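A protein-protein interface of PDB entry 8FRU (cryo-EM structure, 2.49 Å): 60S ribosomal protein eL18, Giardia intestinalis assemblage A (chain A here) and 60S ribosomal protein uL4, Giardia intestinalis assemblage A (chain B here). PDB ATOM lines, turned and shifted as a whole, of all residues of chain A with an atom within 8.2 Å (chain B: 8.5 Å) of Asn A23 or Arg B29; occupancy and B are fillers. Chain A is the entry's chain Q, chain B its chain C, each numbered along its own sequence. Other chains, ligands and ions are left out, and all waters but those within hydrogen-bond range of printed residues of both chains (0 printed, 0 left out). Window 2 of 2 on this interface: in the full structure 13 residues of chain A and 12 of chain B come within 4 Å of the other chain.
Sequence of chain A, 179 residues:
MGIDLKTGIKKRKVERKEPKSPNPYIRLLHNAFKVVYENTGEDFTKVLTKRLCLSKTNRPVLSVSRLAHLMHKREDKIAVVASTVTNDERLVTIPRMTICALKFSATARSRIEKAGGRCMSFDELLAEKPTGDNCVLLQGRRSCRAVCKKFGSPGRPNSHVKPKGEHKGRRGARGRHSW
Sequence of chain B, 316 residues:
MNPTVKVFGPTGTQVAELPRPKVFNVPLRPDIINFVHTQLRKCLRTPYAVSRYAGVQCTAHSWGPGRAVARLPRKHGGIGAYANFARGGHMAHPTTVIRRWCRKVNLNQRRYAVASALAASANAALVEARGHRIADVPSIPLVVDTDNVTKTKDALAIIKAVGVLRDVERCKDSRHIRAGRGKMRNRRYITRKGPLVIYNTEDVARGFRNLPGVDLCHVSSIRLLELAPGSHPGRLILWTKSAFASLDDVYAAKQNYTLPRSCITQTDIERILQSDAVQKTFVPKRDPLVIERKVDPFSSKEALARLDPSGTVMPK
OG of Ser A21 lies within hydrogen-bond range of N of Asn A23, 2.9 Å away.
OD1 of Asn A23 sits close to N of Tyr A25 (3.5 Å).
OD2 of Asp B31 lies within salt-bridge range of NH2 of Arg B29, at 3.1 Å.
OG of Ser B116 sits at hydrogen-bond distance from N of Arg B29, at 3.2 Å.
Asp B31 touches Pro A22.
CZ of Arg B29 touches OD1 of Asn A23 (3.5 Å).
Ile B264 touches Tyr A25 (CG1 to CE1, 3.97 Å).
Of the 12 printed residues of chain A, 3 touch a printed residue of chain B.
Printed residues of chain A that touch a printed residue of chain B: Pro A22, Asn A23 and Tyr A25.
Hydrophobic or aromatic side chains of chain B that line the printed part of chain A: Ile B264.
Among the printed residues, no Asp or Glu carboxylate lies within 4 Å of a Lys or Arg side-chain nitrogen of the other chain.
Printed residues of chain B within 4 Å of Asn A23: Arg B29.
Of chain A, only Asn A23 (3.5 Å) comes within 4 Å of Arg B29.
No residue of chain B comes within 4 Å of Pro A24.
Of the printed residues of chain B, Tyr A25 touches Ile B264.
Of the printed residues of chain A, Ile B264 touches Tyr A25 (3.97 Å).
Of the printed residues of chain A, Asp B31 touches Pro A22 (3.8 Å).
Val B36 touches none of the printed residues of chain A.
Asn B34 touches none of the printed residues of chain A.
The nearest residue of chain B that does not touch Asn A23 is Asp B31 (4.3 Å).
The nearest residue of chain A that does not touch Arg B29 is Pro A24 (4.1 Å).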
ATOM      1  N   PRO A  19     -17.407  -7.178 -23.833  1.00  0.00           N
ATOM      2  CA  PRO A  19     -18.554  -7.912 -24.391  1.00  0.00           C
ATOM      3  C   PRO A  19     -19.821  -7.088 -24.546  1.00  0.00           C
ATOM      4  O   PRO A  19     -20.584  -7.340 -25.485  1.00  0.00           O
ATOM      5  CB  PRO A  19     -18.742  -9.061 -23.392  1.00  0.00           C
ATOM      6  CG  PRO A  19     -17.404  -9.242 -22.792  1.00  0.00           C
ATOM      7  CD  PRO A  19     -16.839  -7.864 -22.666  1.00  0.00           C
ATOM      8  N   LYS A  20     -20.091  -6.132 -23.662  1.00  0.00           N
ATOM      9  CA  LYS A  20     -21.274  -5.268 -23.713  1.00  0.00           C
ATOM     10  C   LYS A  20     -22.550  -5.927 -23.196  1.00  0.00           C
ATOM     11  O   LYS A  20     -23.586  -5.265 -23.174  1.00  0.00           O
ATOM     12  CB  LYS A  20     -21.563  -4.750 -25.129  1.00  0.00           C
ATOM     13  CG  LYS A  20     -22.187  -3.380 -25.166  1.00  0.00           C
ATOM     14  CD  LYS A  20     -22.849  -3.116 -26.496  1.00  0.00           C
ATOM     15  CE  LYS A  20     -23.168  -1.647 -26.661  1.00  0.00           C
ATOM     16  NZ  LYS A  20     -21.940  -0.818 -26.753  1.00  0.00           N
ATOM     17  N   SER A  21     -22.518  -7.168 -22.793  1.00  0.00           N
ATOM     18  CA  SER A  21     -23.708  -7.877 -22.359  1.00  0.00           C
ATOM     19  C   SER A  21     -23.821  -7.877 -20.841  1.00  0.00           C
ATOM     20  O   SER A  21     -22.811  -7.902 -20.137  1.00  0.00           O
ATOM     21  CB  SER A  21     -23.680  -9.320 -22.863  1.00  0.00           C
ATOM     22  OG  SER A  21     -24.327 -10.190 -21.961  1.00  0.00           O
ATOM     23  N   PRO A  22     -25.042  -7.844 -20.304  1.00  0.00           N
ATOM     24  CA  PRO A  22     -25.202  -7.928 -18.846  1.00  0.00           C
ATOM     25  C   PRO A  22     -24.940  -9.312 -18.286  1.00  0.00           C
ATOM     26  O   PRO A  22     -24.709  -9.434 -17.080  1.00  0.00           O
ATOM     27  CB  PRO A  22     -26.664  -7.518 -18.626  1.00  0.00           C
ATOM     28  CG  PRO A  22     -27.107  -6.920 -19.907  1.00  0.00           C
ATOM     29  CD  PRO A  22     -26.329  -7.608 -20.968  1.00  0.00           C
ATOM     30  N   ASN A  23     -24.976 -10.349 -19.108  1.00  0.00           N
ATOM     31  CA  ASN A  23     -24.771 -11.703 -18.621  1.00  0.00           C
ATOM     32  C   ASN A  23     -23.411 -11.814 -17.941  1.00  0.00           C
ATOM     33  O   ASN A  23     -22.385 -11.542 -18.580  1.00  0.00           O
ATOM     34  CB  ASN A  23     -24.869 -12.689 -19.779  1.00  0.00           C
ATOM     35  CG  ASN A  23     -25.152 -14.096 -19.322  1.00  0.00           C
ATOM     36  OD1 ASN A  23     -25.047 -14.406 -18.140  1.00  0.00           O
ATOM     37  ND2 ASN A  23     -25.521 -14.958 -20.256  1.00  0.00           N
ATOM     38  N   PRO A  24     -23.351 -12.207 -16.665  1.00  0.00           N
ATOM     39  CA  PRO A  24     -22.050 -12.259 -15.977  1.00  0.00           C
ATOM     40  C   PRO A  24     -21.165 -13.399 -16.447  1.00  0.00           C
ATOM     41  O   PRO A  24     -19.934 -13.298 -16.351  1.00  0.00           O
ATOM     42  CB  PRO A  24     -22.444 -12.416 -14.503  1.00  0.00           C
ATOM     43  CG  PRO A  24     -23.787 -13.036 -14.538  1.00  0.00           C
ATOM     44  CD  PRO A  24     -24.471 -12.537 -15.768  1.00  0.00           C
ATOM     45  N   TYR A  25     -21.757 -14.472 -16.968  1.00  0.00           N
ATOM     46  CA  TYR A  25     -20.975 -15.584 -17.488  1.00  0.00           C
ATOM     47  C   TYR A  25     -20.046 -15.132 -18.610  1.00  0.00           C
ATOM     48  O   TYR A  25     -18.862 -15.494 -18.637  1.00  0.00           O
ATOM     49  CB  TYR A  25     -21.928 -16.668 -17.977  1.00  0.00           C
ATOM     50  CG  TYR A  25     -21.274 -17.933 -18.448  1.00  0.00           C
ATOM     51  CD1 TYR A  25     -20.655 -18.791 -17.554  1.00  0.00           C
ATOM     52  CD2 TYR A  25     -21.295 -18.283 -19.784  1.00  0.00           C
ATOM     53  CE1 TYR A  25     -20.063 -19.953 -17.982  1.00  0.00           C
ATOM     54  CE2 TYR A  25     -20.706 -19.444 -20.222  1.00  0.00           C
ATOM     55  CZ  TYR A  25     -20.090 -20.276 -19.318  1.00  0.00           C
ATOM     56  OH  TYR A  25     -19.499 -21.436 -19.752  1.00  0.00           O
ATOM     57  N   ILE A  26     -20.566 -14.331 -19.538  1.00  0.00           N
ATOM     58  CA  ILE A  26     -19.775 -13.891 -20.677  1.00  0.00           C
ATOM     59  C   ILE A  26     -18.666 -12.944 -20.239  1.00  0.00           C
ATOM     60  O   ILE A  26     -17.553 -12.998 -20.771  1.00  0.00           O
ATOM     61  CB  ILE A  26     -20.705 -13.254 -21.723  1.00  0.00           C
ATOM     62  CG1 ILE A  26     -21.670 -14.308 -22.257  1.00  0.00           C
ATOM     63  CG2 ILE A  26     -19.913 -12.642 -22.855  1.00  0.00           C
ATOM     64  CD1 ILE A  26     -23.098 -13.853 -22.285  1.00  0.00           C
ATOM     65  N   ARG A  27     -18.935 -12.081 -19.258  1.00  0.00           N
ATOM     66  CA  ARG A  27     -17.881 -11.224 -18.730  1.00  0.00           C
ATOM     67  C   ARG A  27     -16.767 -12.051 -18.103  1.00  0.00           C
ATOM     68  O   ARG A  27     -15.577 -11.787 -18.328  1.00  0.00           O
ATOM     69  CB  ARG A  27     -18.455 -10.250 -17.701  1.00  0.00           C
ATOM     70  CG  ARG A  27     -19.758  -9.599 -18.094  1.00  0.00           C
ATOM     71  CD  ARG A  27     -19.581  -8.720 -19.308  1.00  0.00           C
ATOM     72  NE  ARG A  27     -20.482  -7.574 -19.297  1.00  0.00           N
ATOM     73  CZ  ARG A  27     -20.101  -6.323 -19.080  1.00  0.00           C
ATOM     74  NH1 ARG A  27     -18.837  -6.017 -18.839  1.00  0.00           N
ATOM     75  NH2 ARG A  27     -21.011  -5.355 -19.105  1.00  0.00           N
ATOM     76  N   LEU A  28     -17.136 -13.058 -17.305  1.00  0.00           N
ATOM     77  CA  LEU A  28     -16.130 -13.904 -16.669  1.00  0.00           C
ATOM     78  C   LEU A  28     -15.269 -14.604 -17.709  1.00  0.00           C
ATOM     79  O   LEU A  28     -14.035 -14.610 -17.614  1.00  0.00           O
ATOM     80  CB  LEU A  28     -16.805 -14.930 -15.764  1.00  0.00           C
ATOM     81  CG  LEU A  28     -17.320 -14.440 -14.411  1.00  0.00           C
ATOM     82  CD1 LEU A  28     -18.011 -15.570 -13.672  1.00  0.00           C
ATOM     83  CD2 LEU A  28     -16.182 -13.876 -13.582  1.00  0.00           C
ATOM     84  N   LEU A  29     -15.906 -15.193 -18.719  1.00  0.00           N
ATOM     85  CA  LEU A  29     -15.146 -15.898 -19.744  1.00  0.00           C
ATOM     86  C   LEU A  29     -14.222 -14.953 -20.499  1.00  0.00           C
ATOM     87  O   LEU A  29     -13.056 -15.285 -20.756  1.00  0.00           O
ATOM     88  CB  LEU A  29     -16.095 -16.603 -20.709  1.00  0.00           C
ATOM     89  CG  LEU A  29     -16.628 -17.958 -20.264  1.00  0.00           C
ATOM     90  CD1 LEU A  29     -17.502 -18.541 -21.352  1.00  0.00           C
ATOM     91  CD2 LEU A  29     -15.490 -18.893 -19.932  1.00  0.00           C
ATOM     92  N   LEU A 102     -21.036 -22.008 -26.797  1.00  0.00           N
ATOM     93  CA  LEU A 102     -21.636 -21.193 -25.747  1.00  0.00           C
ATOM     94  C   LEU A 102     -22.934 -21.806 -25.246  1.00  0.00           C
ATOM     95  O   LEU A 102     -23.251 -21.710 -24.057  1.00  0.00           O
ATOM     96  CB  LEU A 102     -21.887 -19.777 -26.257  1.00  0.00           C
ATOM     97  CG  LEU A 102     -20.749 -18.766 -26.173  1.00  0.00           C
ATOM     98  CD1 LEU A 102     -21.319 -17.377 -26.298  1.00  0.00           C
ATOM     99  CD2 LEU A 102     -19.983 -18.915 -24.877  1.00  0.00           C
ATOM    100  N   VAL B  26     -30.276 -23.070  -9.778  1.00  0.00           N
ATOM    101  CA  VAL B  26     -30.384 -22.190 -10.936  1.00  0.00           C
ATOM    102  C   VAL B  26     -29.337 -21.088 -10.834  1.00  0.00           C
ATOM    103  O   VAL B  26     -28.943 -20.710  -9.723  1.00  0.00           O
ATOM    104  CB  VAL B  26     -31.807 -21.623 -11.055  1.00  0.00           C
ATOM    105  CG1 VAL B  26     -31.820 -20.346 -11.863  1.00  0.00           C
ATOM    106  CG2 VAL B  26     -32.724 -22.655 -11.691  1.00  0.00           C
ATOM    107  N   PRO B  27     -28.841 -20.568 -11.954  1.00  0.00           N
ATOM    108  CA  PRO B  27     -27.876 -19.464 -11.893  1.00  0.00           C
ATOM    109  C   PRO B  27     -28.506 -18.187 -11.361  1.00  0.00           C
ATOM    110  O   PRO B  27     -29.702 -17.939 -11.525  1.00  0.00           O
ATOM    111  CB  PRO B  27     -27.442 -19.290 -13.353  1.00  0.00           C
ATOM    112  CG  PRO B  27     -27.875 -20.527 -14.048  1.00  0.00           C
ATOM    113  CD  PRO B  27     -29.072 -21.025 -13.329  1.00  0.00           C
ATOM    114  N   LEU B  28     -27.676 -17.362 -10.735  1.00  0.00           N
ATOM    115  CA  LEU B  28     -28.108 -16.066 -10.224  1.00  0.00           C
ATOM    116  C   LEU B  28     -27.925 -15.006 -11.304  1.00  0.00           C
ATOM    117  O   LEU B  28     -26.798 -14.714 -11.707  1.00  0.00           O
ATOM    118  CB  LEU B  28     -27.322 -15.696  -8.969  1.00  0.00           C
ATOM    119  CG  LEU B  28     -27.247 -16.783  -7.899  1.00  0.00           C
ATOM    120  CD1 LEU B  28     -26.508 -16.283  -6.671  1.00  0.00           C
ATOM    121  CD2 LEU B  28     -28.636 -17.280  -7.530  1.00  0.00           C
ATOM    122  N   ARG B  29     -29.034 -14.428 -11.763  1.00  0.00           N
ATOM    123  CA  ARG B  29     -29.040 -13.426 -12.827  1.00  0.00           C
ATOM    124  C   ARG B  29     -29.715 -12.159 -12.318  1.00  0.00           C
ATOM    125  O   ARG B  29     -30.937 -12.007 -12.441  1.00  0.00           O
ATOM    126  CB  ARG B  29     -29.749 -13.954 -14.070  1.00  0.00           C
ATOM    127  CG  ARG B  29     -29.269 -15.307 -14.542  1.00  0.00           C
ATOM    128  CD  ARG B  29     -28.054 -15.187 -15.438  1.00  0.00           C
ATOM    129  NE  ARG B  29     -28.187 -14.118 -16.417  1.00  0.00           N
ATOM    130  CZ  ARG B  29     -28.561 -14.297 -17.676  1.00  0.00           C
ATOM    131  NH1 ARG B  29     -28.844 -15.498 -18.146  1.00  0.00           N
ATOM    132  NH2 ARG B  29     -28.652 -13.245 -18.482  1.00  0.00           N
ATOM    133  N   PRO B  30     -28.961 -11.224 -11.742  1.00  0.00           N
ATOM    134  CA  PRO B  30     -29.579  -9.964 -11.303  1.00  0.00           C
ATOM    135  C   PRO B  30     -30.227  -9.181 -12.428  1.00  0.00           C
ATOM    136  O   PRO B  30     -31.252  -8.529 -12.204  1.00  0.00           O
ATOM    137  CB  PRO B  30     -28.402  -9.195 -10.685  1.00  0.00           C
ATOM    138  CG  PRO B  30     -27.375 -10.222 -10.398  1.00  0.00           C
ATOM    139  CD  PRO B  30     -27.524 -11.268 -11.440  1.00  0.00           C
ATOM    140  N   ASP B  31     -29.664  -9.224 -13.637  1.00  0.00           N
ATOM    141  CA  ASP B  31     -30.216  -8.444 -14.740  1.00  0.00           C
ATOM    142  C   ASP B  31     -31.618  -8.911 -15.111  1.00  0.00           C
ATOM    143  O   ASP B  31     -32.517  -8.087 -15.322  1.00  0.00           O
ATOM    144  CB  ASP B  31     -29.283  -8.514 -15.948  1.00  0.00           C
ATOM    145  CG  ASP B  31     -28.860  -9.931 -16.286  1.00  0.00           C
ATOM    146  OD1 ASP B  31     -28.451 -10.671 -15.371  1.00  0.00           O
ATOM    147  OD2 ASP B  31     -28.929 -10.303 -17.474  1.00  0.00           O
ATOM    148  N   ILE B  32     -31.827 -10.227 -15.188  1.00  0.00           N
ATOM    149  CA  ILE B  32     -33.142 -10.763 -15.533  1.00  0.00           C
ATOM    150  C   ILE B  32     -34.157 -10.444 -14.443  1.00  0.00           C
ATOM    151  O   ILE B  32     -35.301 -10.065 -14.731  1.00  0.00           O
ATOM    152  CB  ILE B  32     -33.045 -12.277 -15.794  1.00  0.00           C
ATOM    153  CG1 ILE B  32     -32.259 -12.548 -17.074  1.00  0.00           C
ATOM    154  CG2 ILE B  32     -34.428 -12.903 -15.860  1.00  0.00           C
ATOM    155  CD1 ILE B  32     -32.299 -13.979 -17.528  1.00  0.00           C
ATOM    156  N   ILE B  33     -33.764 -10.598 -13.180  1.00  0.00           N
ATOM    157  CA  ILE B  33     -34.669 -10.279 -12.083  1.00  0.00           C
ATOM    158  C   ILE B  33     -35.063  -8.811 -12.135  1.00  0.00           C
ATOM    159  O   ILE B  33     -36.236  -8.465 -11.968  1.00  0.00           O
ATOM    160  CB  ILE B  33     -34.032 -10.651 -10.733  1.00  0.00           C
ATOM    161  CG1 ILE B  33     -33.897 -12.165 -10.606  1.00  0.00           C
ATOM    162  CG2 ILE B  33     -34.860 -10.117  -9.590  1.00  0.00           C
ATOM    163  CD1 ILE B  33     -32.983 -12.595  -9.504  1.00  0.00           C
ATOM    164  N   ASN B  34     -34.096  -7.928 -12.383  1.00  0.00           N
ATOM    165  CA  ASN B  34     -34.395  -6.504 -12.466  1.00  0.00           C
ATOM    166  C   ASN B  34     -35.355  -6.203 -13.610  1.00  0.00           C
ATOM    167  O   ASN B  34     -36.323  -5.451 -13.441  1.00  0.00           O
ATOM    168  CB  ASN B  34     -33.097  -5.718 -12.629  1.00  0.00           C
ATOM    169  CG  ASN B  34     -33.225  -4.287 -12.180  1.00  0.00           C
ATOM    170  OD1 ASN B  34     -33.419  -4.013 -11.002  1.00  0.00           O
ATOM    171  ND2 ASN B  34     -33.114  -3.362 -13.117  1.00  0.00           N
ATOM    172  N   PHE B  35     -35.106  -6.785 -14.782  1.00  0.00           N
ATOM    173  CA  PHE B  35     -35.959  -6.521 -15.937  1.00  0.00           C
ATOM    174  C   PHE B  35     -37.396  -6.949 -15.666  1.00  0.00           C
ATOM    175  O   PHE B  35     -38.348  -6.190 -15.909  1.00  0.00           O
ATOM    176  CB  PHE B  35     -35.396  -7.242 -17.161  1.00  0.00           C
ATOM    177  CG  PHE B  35     -36.334  -7.285 -18.327  1.00  0.00           C
ATOM    178  CD1 PHE B  35     -36.502  -6.183 -19.138  1.00  0.00           C
ATOM    179  CD2 PHE B  35     -37.040  -8.432 -18.619  1.00  0.00           C
ATOM    180  CE1 PHE B  35     -37.362  -6.222 -20.206  1.00  0.00           C
ATOM    181  CE2 PHE B  35     -37.903  -8.475 -19.684  1.00  0.00           C
ATOM    182  CZ  PHE B  35     -38.064  -7.369 -20.478  1.00  0.00           C
ATOM    183  N   VAL B  36     -37.570  -8.160 -15.137  1.00  0.00           N
ATOM    184  CA  VAL B  36     -38.918  -8.663 -14.909  1.00  0.00           C
ATOM    185  C   VAL B  36     -39.604  -7.882 -13.797  1.00  0.00           C
ATOM    186  O   VAL B  36     -40.809  -7.619 -13.863  1.00  0.00           O
ATOM    187  CB  VAL B  36     -38.885 -10.173 -14.623  1.00  0.00           C
ATOM    188  CG1 VAL B  36     -40.270 -10.677 -14.301  1.00  0.00           C
ATOM    189  CG2 VAL B  36     -38.330 -10.914 -15.823  1.00  0.00           C
ATOM    190  N   GLN B 109     -39.336 -16.158 -19.367  1.00  0.00           N
ATOM    191  CA  GLN B 109     -38.527 -15.223 -18.594  1.00  0.00           C
ATOM    192  C   GLN B 109     -39.130 -14.939 -17.220  1.00  0.00           C
ATOM    193  O   GLN B 109     -38.388 -14.745 -16.254  1.00  0.00           O
ATOM    194  CB  GLN B 109     -38.330 -13.941 -19.396  1.00  0.00           C
ATOM    195  CG  GLN B 109     -38.091 -14.226 -20.862  1.00  0.00           C
ATOM    196  CD  GLN B 109     -37.483 -13.068 -21.624  1.00  0.00           C
ATOM    197  OE1 GLN B 109     -38.015 -12.652 -22.644  1.00  0.00           O
ATOM    198  NE2 GLN B 109     -36.365 -12.556 -21.146  1.00  0.00           N
ATOM    199  N   TYR B 112     -38.033 -17.948 -15.274  1.00  0.00           N
ATOM    200  CA  TYR B 112     -36.612 -17.804 -14.980  1.00  0.00           C
ATOM    201  C   TYR B 112     -36.387 -16.852 -13.814  1.00  0.00           C
ATOM    202  O   TYR B 112     -35.600 -17.140 -12.906  1.00  0.00           O
ATOM    203  CB  TYR B 112     -35.882 -17.312 -16.231  1.00  0.00           C
ATOM    204  CG  TYR B 112     -34.396 -17.585 -16.269  1.00  0.00           C
ATOM    205  CD1 TYR B 112     -33.618 -17.474 -15.127  1.00  0.00           C
ATOM    206  CD2 TYR B 112     -33.768 -17.933 -17.452  1.00  0.00           C
ATOM    207  CE1 TYR B 112     -32.268 -17.715 -15.159  1.00  0.00           C
ATOM    208  CE2 TYR B 112     -32.416 -18.175 -17.493  1.00  0.00           C
ATOM    209  CZ  TYR B 112     -31.671 -18.061 -16.342  1.00  0.00           C
ATOM    210  OH  TYR B 112     -30.323 -18.301 -16.371  1.00  0.00           O
ATOM    211  N   ALA B 113     -37.062 -15.702 -13.826  1.00  0.00           N
ATOM    212  CA  ALA B 113     -36.867 -14.723 -12.765  1.00  0.00           C
ATOM    213  C   ALA B 113     -37.285 -15.275 -11.409  1.00  0.00           C
ATOM    214  O   ALA B 113     -36.571 -15.103 -10.412  1.00  0.00           O
ATOM    215  CB  ALA B 113     -37.637 -13.444 -13.081  1.00  0.00           C
ATOM    216  N   ALA B 115     -37.448 -18.413 -10.445  1.00  0.00           N
ATOM    217  CA  ALA B 115     -36.516 -19.457 -10.025  1.00  0.00           C
ATOM    218  C   ALA B 115     -35.204 -18.865  -9.527  1.00  0.00           C
ATOM    219  O   ALA B 115     -34.653 -19.315  -8.516  1.00  0.00           O
ATOM    220  CB  ALA B 115     -36.266 -20.430 -11.174  1.00  0.00           C
ATOM    221  N   SER B 116     -34.683 -17.858 -10.226  1.00  0.00           N
ATOM    222  CA  SER B 116     -33.430 -17.237  -9.813  1.00  0.00           C
ATOM    223  C   SER B 116     -33.571 -16.536  -8.467  1.00  0.00           C
ATOM    224  O   SER B 116     -32.654 -16.582  -7.639  1.00  0.00           O
ATOM    225  CB  SER B 116     -32.961 -16.261 -10.887  1.00  0.00           C
ATOM    226  OG  SER B 116     -31.559 -16.116 -10.883  1.00  0.00           O
ATOM    227  N   ALA B 117     -34.708 -15.877  -8.228  1.00  0.00           N
ATOM    228  CA  ALA B 117     -34.929 -15.254  -6.926  1.00  0.00           C
ATOM    229  C   ALA B 117     -35.027 -16.295  -5.818  1.00  0.00           C
ATOM    230  O   ALA B 117     -34.489 -16.099  -4.721  1.00  0.00           O
ATOM    231  CB  ALA B 117     -36.182 -14.386  -6.964  1.00  0.00           C
ATOM    232  N   ALA B 119     -33.498 -19.170  -5.826  1.00  0.00           N
ATOM    233  CA  ALA B 119     -32.138 -19.648  -5.607  1.00  0.00           C
ATOM    234  C   ALA B 119     -31.319 -18.639  -4.816  1.00  0.00           C
ATOM    235  O   ALA B 119     -30.452 -19.018  -4.023  1.00  0.00           O
ATOM    236  CB  ALA B 119     -31.467 -19.958  -6.942  1.00  0.00           C
ATOM    237  N   ALA B 120     -31.563 -17.347  -5.033  1.00  0.00           N
ATOM    238  CA  ALA B 120     -30.889 -16.327  -4.238  1.00  0.00           C
ATOM    239  C   ALA B 120     -31.332 -16.356  -2.783  1.00  0.00           C
ATOM    240  O   ALA B 120     -30.549 -16.018  -1.892  1.00  0.00           O
ATOM    241  CB  ALA B 120     -31.138 -14.942  -4.827  1.00  0.00           C
ATOM    242  N   LEU B 126     -26.250 -13.364   0.495  1.00  0.00           N
ATOM    243  CA  LEU B 126     -27.178 -12.427  -0.127  1.00  0.00           C
ATOM    244  C   LEU B 126     -28.270 -12.000   0.845  1.00  0.00           C
ATOM    245  O   LEU B 126     -28.705 -10.843   0.828  1.00  0.00           O
ATOM    246  CB  LEU B 126     -27.787 -13.049  -1.379  1.00  0.00           C
ATOM    247  CG  LEU B 126     -27.146 -12.637  -2.701  1.00  0.00           C
ATOM    248  CD1 LEU B 126     -25.639 -12.606  -2.572  1.00  0.00           C
ATOM    249  CD2 LEU B 126     -27.563 -13.590  -3.792  1.00  0.00           C
ATOM    250  N   SER B 231     -36.565  -4.718  -5.885  1.00  0.00           N
ATOM    251  CA  SER B 231     -35.728  -5.311  -6.918  1.00  0.00           C
ATOM    252  C   SER B 231     -34.441  -5.905  -6.361  1.00  0.00           C
ATOM    253  O   SER B 231     -33.510  -6.169  -7.120  1.00  0.00           O
ATOM    254  CB  SER B 231     -35.410  -4.299  -8.022  1.00  0.00           C
ATOM    255  OG  SER B 231     -34.074  -4.416  -8.464  1.00  0.00           O
ATOM    256  N   PRO B 233     -32.799  -9.173  -4.473  1.00  0.00           N
ATOM    257  CA  PRO B 233     -33.326 -10.545  -4.496  1.00  0.00           C
ATOM    258  C   PRO B 233     -33.314 -11.332  -3.192  1.00  0.00           C
ATOM    259  O   PRO B 233     -34.189 -12.181  -3.002  1.00  0.00           O
ATOM    260  CB  PRO B 233     -32.429 -11.229  -5.538  1.00  0.00           C
ATOM    261  CG  PRO B 233     -31.799 -10.121  -6.300  1.00  0.00           C
ATOM    262  CD  PRO B 233     -31.600  -9.043  -5.306  1.00  0.00           C
ATOM    263  N   PRO B 260     -33.364 -23.896 -16.136  1.00  0.00           N
ATOM    264  CA  PRO B 260     -32.113 -23.530 -16.810  1.00  0.00           C
ATOM    265  C   PRO B 260     -30.901 -24.195 -16.173  1.00  0.00           C
ATOM    266  O   PRO B 260     -30.853 -24.431 -14.965  1.00  0.00           O
ATOM    267  CB  PRO B 260     -32.059 -22.004 -16.662  1.00  0.00           C
ATOM    268  CG  PRO B 260     -33.057 -21.664 -15.614  1.00  0.00           C
ATOM    269  CD  PRO B 260     -34.096 -22.723 -15.637  1.00  0.00           C
ATOM    270  N   ARG B 261     -29.911 -24.492 -17.012  1.00  0.00           N
ATOM    271  CA  ARG B 261     -28.733 -25.234 -16.583  1.00  0.00           C
ATOM    272  C   ARG B 261     -27.849 -24.403 -15.663  1.00  0.00           C
ATOM    273  O   ARG B 261     -27.691 -23.194 -15.838  1.00  0.00           O
ATOM    274  CB  ARG B 261     -27.916 -25.679 -17.792  1.00  0.00           C
ATOM    275  CG  ARG B 261     -28.383 -26.963 -18.427  1.00  0.00           C
ATOM    276  CD  ARG B 261     -27.560 -27.274 -19.656  1.00  0.00           C
ATOM    277  NE  ARG B 261     -26.301 -27.914 -19.304  1.00  0.00           N
ATOM    278  CZ  ARG B 261     -26.141 -29.223 -19.171  1.00  0.00           C
ATOM    279  NH1 ARG B 261     -27.137 -30.065 -19.389  1.00  0.00           N
ATOM    280  NH2 ARG B 261     -24.955 -29.697 -18.803  1.00  0.00           N
ATOM    281  N   CYS B 263     -24.328 -23.070 -14.012  1.00  0.00           N
ATOM    282  CA  CYS B 263     -23.070 -22.618 -14.588  1.00  0.00           C
ATOM    283  C   CYS B 263     -22.100 -22.281 -13.462  1.00  0.00           C
ATOM    284  O   CYS B 263     -22.452 -22.310 -12.280  1.00  0.00           O
ATOM    285  CB  CYS B 263     -23.283 -21.418 -15.514  1.00  0.00           C
ATOM    286  SG  CYS B 263     -23.888 -19.940 -14.676  1.00  0.00           S
ATOM    287  N   ILE B 264     -20.866 -21.954 -13.842  1.00  0.00           N
ATOM    288  CA  ILE B 264     -19.821 -21.655 -12.872  1.00  0.00           C
ATOM    289  C   ILE B 264     -19.927 -20.202 -12.419  1.00  0.00           C
ATOM    290  O   ILE B 264     -20.519 -19.352 -13.086  1.00  0.00           O
ATOM    291  CB  ILE B 264     -18.433 -21.948 -13.460  1.00  0.00           C
ATOM    292  CG1 ILE B 264     -18.175 -21.040 -14.663  1.00  0.00           C
ATOM    293  CG2 ILE B 264     -18.319 -23.406 -13.855  1.00  0.00           C
ATOM    294  CD1 ILE B 264     -16.720 -20.769 -14.911  1.00  0.00           C
